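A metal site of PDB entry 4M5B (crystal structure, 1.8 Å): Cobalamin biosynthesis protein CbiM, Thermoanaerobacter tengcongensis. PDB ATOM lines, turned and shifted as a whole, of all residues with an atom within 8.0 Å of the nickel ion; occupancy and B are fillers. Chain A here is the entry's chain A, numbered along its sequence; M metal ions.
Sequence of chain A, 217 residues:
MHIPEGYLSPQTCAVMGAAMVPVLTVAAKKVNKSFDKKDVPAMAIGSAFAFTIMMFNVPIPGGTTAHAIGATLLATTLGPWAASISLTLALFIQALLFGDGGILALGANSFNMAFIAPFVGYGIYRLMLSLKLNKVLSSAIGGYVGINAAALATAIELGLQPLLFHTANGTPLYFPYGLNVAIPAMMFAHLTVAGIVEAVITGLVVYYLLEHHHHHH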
ATOM      1  N   MET A   1      26.305  30.695 -17.142  1.00  0.00           N
ATOM      2  CA  MET A   1      27.400  30.718 -18.118  1.00  0.00           C
ATOM      3  C   MET A   1      27.886  29.359 -18.694  1.00  0.00           C
ATOM      4  O   MET A   1      28.634  29.352 -19.666  1.00  0.00           O
ATOM      5  CB  MET A   1      28.579  31.511 -17.539  1.00  0.00           C
ATOM      6  CG  MET A   1      29.308  30.857 -16.360  1.00  0.00           C
ATOM      7  SD  MET A   1      30.597  31.981 -15.774  1.00  0.00           S
ATOM      8  CE  MET A   1      29.600  33.158 -14.853  1.00  0.00           C
ATOM      9  N   HIS A   2      27.464  28.236 -18.099  1.00  0.00           N
ATOM     10  CA  HIS A   2      27.786  26.874 -18.480  1.00  0.00           C
ATOM     11  C   HIS A   2      27.729  26.828 -19.980  1.00  0.00           C
ATOM     12  O   HIS A   2      26.710  27.181 -20.592  1.00  0.00           O
ATOM     13  CB  HIS A   2      26.719  25.862 -17.993  1.00  0.00           C
ATOM     14  CG  HIS A   2      26.812  25.458 -16.540  1.00  0.00           C
ATOM     15  ND1 HIS A   2      26.622  26.340 -15.501  1.00  0.00           N
ATOM     16  CD2 HIS A   2      26.993  24.246 -15.958  1.00  0.00           C
ATOM     17  CE1 HIS A   2      26.715  25.706 -14.348  1.00  0.00           C
ATOM     18  NE2 HIS A   2      26.931  24.438 -14.599  1.00  0.00           N
ATOM     19  N   ILE A   3      28.829  26.393 -20.559  1.00  0.00           N
ATOM     20  CA  ILE A   3      28.902  26.156 -21.993  1.00  0.00           C
ATOM     21  C   ILE A   3      28.383  24.741 -22.294  1.00  0.00           C
ATOM     22  O   ILE A   3      28.920  23.750 -21.773  1.00  0.00           O
ATOM     23  CB  ILE A   3      30.359  26.296 -22.417  1.00  0.00           C
ATOM     24  CG1 ILE A   3      30.856  27.713 -22.053  1.00  0.00           C
ATOM     25  CG2 ILE A   3      30.513  26.043 -23.907  1.00  0.00           C
ATOM     26  CD1 ILE A   3      32.365  27.857 -22.129  1.00  0.00           C
ATOM     27  N   PRO A   4      27.327  24.643 -23.130  1.00  0.00           N
ATOM     28  CA  PRO A   4      26.810  23.339 -23.570  1.00  0.00           C
ATOM     29  C   PRO A   4      27.762  22.620 -24.503  1.00  0.00           C
ATOM     30  O   PRO A   4      28.684  23.234 -25.046  1.00  0.00           O
ATOM     31  CB  PRO A   4      25.521  23.707 -24.343  1.00  0.00           C
ATOM     32  CG  PRO A   4      25.126  25.057 -23.815  1.00  0.00           C
ATOM     33  CD  PRO A   4      26.456  25.757 -23.557  1.00  0.00           C
ATOM     34  N   MET A  54      22.909  27.290  -8.962  1.00  0.00           N
ATOM     35  CA  MET A  54      23.120  27.384 -10.411  1.00  0.00           C
ATOM     36  C   MET A  54      21.944  26.894 -11.236  1.00  0.00           C
ATOM     37  O   MET A  54      21.858  27.201 -12.411  1.00  0.00           O
ATOM     38  CB  MET A  54      24.375  26.613 -10.811  1.00  0.00           C
ATOM     39  CG  MET A  54      25.640  27.209 -10.246  1.00  0.00           C
ATOM     40  SD  MET A  54      27.108  26.388 -10.878  1.00  0.00           S
ATOM     41  CE  MET A  54      27.156  24.885  -9.920  1.00  0.00           C
ATOM     42  N   ASN A  57      18.461  29.650 -13.617  1.00  0.00           N
ATOM     43  CA  ASN A  57      19.189  30.373 -14.643  1.00  0.00           C
ATOM     44  C   ASN A  57      18.267  30.865 -15.743  1.00  0.00           C
ATOM     45  O   ASN A  57      17.143  30.359 -15.887  1.00  0.00           O
ATOM     46  CB  ASN A  57      20.305  29.498 -15.217  1.00  0.00           C
ATOM     47  CG  ASN A  57      19.779  28.152 -15.723  1.00  0.00           C
ATOM     48  OD1 ASN A  57      19.203  28.078 -16.803  1.00  0.00           O
ATOM     49  ND2 ASN A  57      19.979  27.104 -14.945  1.00  0.00           N
ATOM     50  N   VAL A  58      18.734  31.844 -16.515  1.00  0.00           N
ATOM     51  CA  VAL A  58      18.005  32.382 -17.654  1.00  0.00           C
ATOM     52  C   VAL A  58      18.942  32.440 -18.866  1.00  0.00           C
ATOM     53  O   VAL A  58      20.148  32.645 -18.716  1.00  0.00           O
ATOM     54  CB  VAL A  58      17.442  33.796 -17.376  1.00  0.00           C
ATOM     55  CG1 VAL A  58      16.338  33.731 -16.326  1.00  0.00           C
ATOM     56  CG2 VAL A  58      18.547  34.751 -16.954  1.00  0.00           C
ATOM     57  N   THR A  64      25.456  32.263 -23.320  1.00  0.00           N
ATOM     58  CA  THR A  64      24.916  30.998 -22.825  1.00  0.00           C
ATOM     59  C   THR A  64      23.754  31.265 -21.862  1.00  0.00           C
ATOM     60  O   THR A  64      22.631  31.460 -22.301  1.00  0.00           O
ATOM     61  CB  THR A  64      25.998  30.126 -22.182  1.00  0.00           C
ATOM     62  OG1 THR A  64      26.739  30.892 -21.214  1.00  0.00           O
ATOM     63  CG2 THR A  64      26.991  29.640 -23.255  1.00  0.00           C
ATOM     64  N   THR A  65      24.049  31.288 -20.558  1.00  0.00           N
ATOM     65  CA  THR A  65      23.028  31.564 -19.542  1.00  0.00           C
ATOM     66  C   THR A  65      23.595  32.448 -18.426  1.00  0.00           C
ATOM     67  O   THR A  65      24.801  32.623 -18.312  1.00  0.00           O
ATOM     68  CB  THR A  65      22.539  30.270 -18.843  1.00  0.00           C
ATOM     69  OG1 THR A  65      23.664  29.580 -18.260  1.00  0.00           O
ATOM     70  CG2 THR A  65      21.815  29.343 -19.827  1.00  0.00           C
ATOM     71  N   ALA A  66      22.701  32.988 -17.591  1.00  0.00           N
ATOM     72  CA  ALA A  66      23.110  33.724 -16.398  1.00  0.00           C
ATOM     73  C   ALA A  66      22.482  33.100 -15.161  1.00  0.00           C
ATOM     74  O   ALA A  66      21.339  32.673 -15.190  1.00  0.00           O
ATOM     75  CB  ALA A  66      22.684  35.192 -16.504  1.00  0.00           C
ATOM     76  N   HIS A  67      23.246  33.046 -14.074  1.00  0.00           N
ATOM     77  CA  HIS A  67      22.754  32.568 -12.788  1.00  0.00           C
ATOM     78  C   HIS A  67      23.854  32.821 -11.776  1.00  0.00           C
ATOM     79  O   HIS A  67      25.006  33.058 -12.143  1.00  0.00           O
ATOM     80  CB  HIS A  67      22.495  31.071 -12.845  1.00  0.00           C
ATOM     81  CG  HIS A  67      23.688  30.302 -13.263  1.00  0.00           C
ATOM     82  ND1 HIS A  67      24.769  30.076 -12.421  1.00  0.00           N
ATOM     83  CD2 HIS A  67      24.029  29.746 -14.453  1.00  0.00           C
ATOM     84  CE1 HIS A  67      25.702  29.415 -13.069  1.00  0.00           C
ATOM     85  NE2 HIS A  67      25.260  29.187 -14.297  1.00  0.00           N
ATOM     86  N   ALA A  68      23.520  32.761 -10.491  1.00  0.00           N
ATOM     87  CA  ALA A  68      24.543  32.910  -9.472  1.00  0.00           C
ATOM     88  C   ALA A  68      25.284  31.580  -9.356  1.00  0.00           C
ATOM     89  O   ALA A  68      24.854  30.572  -9.946  1.00  0.00           O
ATOM     90  CB  ALA A  68      23.916  33.305  -8.145  1.00  0.00           C
ATOM     91  N   ILE A  69      26.397  31.586  -8.618  1.00  0.00           N
ATOM     92  CA  ILE A  69      27.187  30.380  -8.430  1.00  0.00           C
ATOM     93  C   ILE A  69      27.506  30.081  -6.958  1.00  0.00           C
ATOM     94  O   ILE A  69      27.445  28.928  -6.521  1.00  0.00           O
ATOM     95  CB  ILE A  69      28.491  30.447  -9.214  1.00  0.00           C
ATOM     96  CG1 ILE A  69      28.211  30.495 -10.710  1.00  0.00           C
ATOM     97  CG2 ILE A  69      29.389  29.261  -8.893  1.00  0.00           C
ATOM     98  CD1 ILE A  69      29.365  31.097 -11.478  1.00  0.00           C
ATOM     99  N   LEU A  91      29.578  21.012 -10.860  1.00  0.00           N
ATOM    100  CA  LEU A  91      29.565  21.052 -12.324  1.00  0.00           C
ATOM    101  C   LEU A  91      29.571  19.654 -12.930  1.00  0.00           C
ATOM    102  O   LEU A  91      28.901  19.410 -13.938  1.00  0.00           O
ATOM    103  CB  LEU A  91      30.773  21.827 -12.842  1.00  0.00           C
ATOM    104  CG  LEU A  91      30.791  23.294 -12.400  1.00  0.00           C
ATOM    105  CD1 LEU A  91      32.120  23.915 -12.736  1.00  0.00           C
ATOM    106  CD2 LEU A  91      29.663  24.043 -13.083  1.00  0.00           C
ATOM    107  N   GLN A  94      26.092  18.265 -12.598  1.00  0.00           N
ATOM    108  CA  GLN A  94      25.267  18.966 -13.581  1.00  0.00           C
ATOM    109  C   GLN A  94      25.469  18.410 -14.997  1.00  0.00           C
ATOM    110  O   GLN A  94      24.495  18.115 -15.717  1.00  0.00           O
ATOM    111  CB  GLN A  94      25.584  20.458 -13.537  1.00  0.00           C
ATOM    112  CG  GLN A  94      24.951  21.143 -12.345  1.00  0.00           C
ATOM    113  CD  GLN A  94      25.426  22.592 -12.185  1.00  0.00           C
ATOM    114  OE1 GLN A  94      26.510  22.959 -12.649  1.00  0.00           O
ATOM    115  NE2 GLN A  94      24.629  23.410 -11.507  1.00  0.00           N
ATOM    116  N   ASP A 100      23.487  19.694 -18.027  1.00  0.00           N
ATOM    117  CA  ASP A 100      23.699  21.127 -17.883  1.00  0.00           C
ATOM    118  C   ASP A 100      25.210  21.397 -17.933  1.00  0.00           C
ATOM    119  O   ASP A 100      25.931  21.080 -16.992  1.00  0.00           O
ATOM    120  CB  ASP A 100      23.092  21.606 -16.564  1.00  0.00           C
ATOM    121  CG  ASP A 100      23.221  23.115 -16.377  1.00  0.00           C
ATOM    122  OD1 ASP A 100      22.916  23.586 -15.256  1.00  0.00           O
ATOM    123  OD2 ASP A 100      23.606  23.817 -17.324  1.00  0.00           O
ATOM    124  N   GLY A 101      25.665  21.977 -19.041  1.00  0.00           N
ATOM    125  CA  GLY A 101      27.087  22.092 -19.303  1.00  0.00           C
ATOM    126  C   GLY A 101      27.528  20.830 -20.011  1.00  0.00           C
ATOM    127  O   GLY A 101      27.120  19.727 -19.614  1.00  0.00           O
ATOM    128  N   ASN A 109      34.223  24.835 -18.286  1.00  0.00           N
ATOM    129  CA  ASN A 109      33.275  25.304 -17.287  1.00  0.00           C
ATOM    130  C   ASN A 109      33.865  25.323 -15.873  1.00  0.00           C
ATOM    131  O   ASN A 109      33.589  26.224 -15.090  1.00  0.00           O
ATOM    132  CB  ASN A 109      31.991  24.457 -17.332  1.00  0.00           C
ATOM    133  CG  ASN A 109      31.129  24.780 -18.542  1.00  0.00           C
ATOM    134  OD1 ASN A 109      31.041  25.931 -18.951  1.00  0.00           O
ATOM    135  ND2 ASN A 109      30.514  23.755 -19.125  1.00  0.00           N
ATOM    136  N   MET A 113      34.194  28.640 -13.650  1.00  0.00           N
ATOM    137  CA  MET A 113      33.379  28.779 -12.441  1.00  0.00           C
ATOM    138  C   MET A 113      34.017  28.185 -11.208  1.00  0.00           C
ATOM    139  O   MET A 113      33.658  28.533 -10.090  1.00  0.00           O
ATOM    140  CB  MET A 113      31.998  28.145 -12.660  1.00  0.00           C
ATOM    141  CG  MET A 113      31.149  28.893 -13.682  1.00  0.00           C
ATOM    142  SD  MET A 113      29.554  28.127 -13.962  1.00  0.00           S
ATOM    143  CE  MET A 113      29.947  26.964 -15.279  1.00  0.00           C
ATOM    144  N   THR A 154      34.250  33.102 -19.979  1.00  0.00           N
ATOM    145  CA  THR A 154      33.296  32.349 -20.794  1.00  0.00           C
ATOM    146  C   THR A 154      33.073  33.043 -22.138  1.00  0.00           C
ATOM    147  O   THR A 154      33.088  32.403 -23.197  1.00  0.00           O
ATOM    148  CB  THR A 154      31.956  32.211 -20.081  1.00  0.00           C
ATOM    149  OG1 THR A 154      32.142  31.528 -18.830  1.00  0.00           O
ATOM    150  CG2 THR A 154      30.975  31.389 -20.981  1.00  0.00           C
ATOM    151  N   MET A 186      27.245  38.611 -22.482  1.00  0.00           N
ATOM    152  CA  MET A 186      27.501  37.932 -21.204  1.00  0.00           C
ATOM    153  C   MET A 186      27.766  38.939 -20.093  1.00  0.00           C
ATOM    154  O   MET A 186      27.343  38.747 -18.950  1.00  0.00           O
ATOM    155  CB  MET A 186      28.679  36.961 -21.337  1.00  0.00           C
ATOM    156  CG  MET A 186      28.369  35.741 -22.207  1.00  0.00           C
ATOM    157  SD  MET A 186      27.063  34.762 -21.458  1.00  0.00           S
ATOM    158  CE  MET A 186      27.939  34.013 -20.079  1.00  0.00           C
ATOM    159  N   HIS A 190      25.760  39.804 -16.445  1.00  0.00           N
ATOM    160  CA  HIS A 190      26.436  39.493 -15.193  1.00  0.00           C
ATOM    161  C   HIS A 190      26.797  40.752 -14.393  1.00  0.00           C
ATOM    162  O   HIS A 190      26.839  40.719 -13.156  1.00  0.00           O
ATOM    163  CB  HIS A 190      27.652  38.598 -15.451  1.00  0.00           C
ATOM    164  CG  HIS A 190      27.268  37.191 -15.794  1.00  0.00           C
ATOM    165  ND1 HIS A 190      26.866  36.808 -17.056  1.00  0.00           N
ATOM    166  CD2 HIS A 190      27.178  36.073 -15.027  1.00  0.00           C
ATOM    167  CE1 HIS A 190      26.564  35.521 -17.060  1.00  0.00           C
ATOM    168  NE2 HIS A 190      26.752  35.052 -15.837  1.00  0.00           N
HETATM  169 NI    NI M   1      26.354  28.551 -16.198  1.00  0.00          NI
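The nickel ion is bound by N of His 2 (2.2 Å), NE2 of His 67 (2.3 Å), ND1 of His 2 (2.3 Å) and N of Met 1 (2.3 Å).
The nickel ion has four donor atoms within binding distance.
ND1 of His 2 sits close to SD of Met 113, at 3.8 Å.
NE2 of His 2 is in hydrogen-bond range of OE1 of Gln 94 (2.5 Å).
N of Met 1 lies close to O of Thr 65 (2.7 Å).
The backbone carbonyl oxygen of Met 1 sits at hydrogen-bond distance from the side-chain hydroxyl of Thr 64 (2.9 Å).
The side-chain sulfur (SD) of Met 1 is in hydrogen-bond range of the side-chain hydroxyl (OG1) of Thr 154 (3.5 Å).
Thr 65 touches the nickel ion (OG1 to NI, 3.5 Å).
SD of Met 113 touches the nickel ion, at 3.9 Å.
Within 4 Å of the nickel ion: Met 1, His 2, Thr 65, His 67 and Met 113.
The nearest printed residue that does not touch the nickel ion is Ile 3 (5.5 Å).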
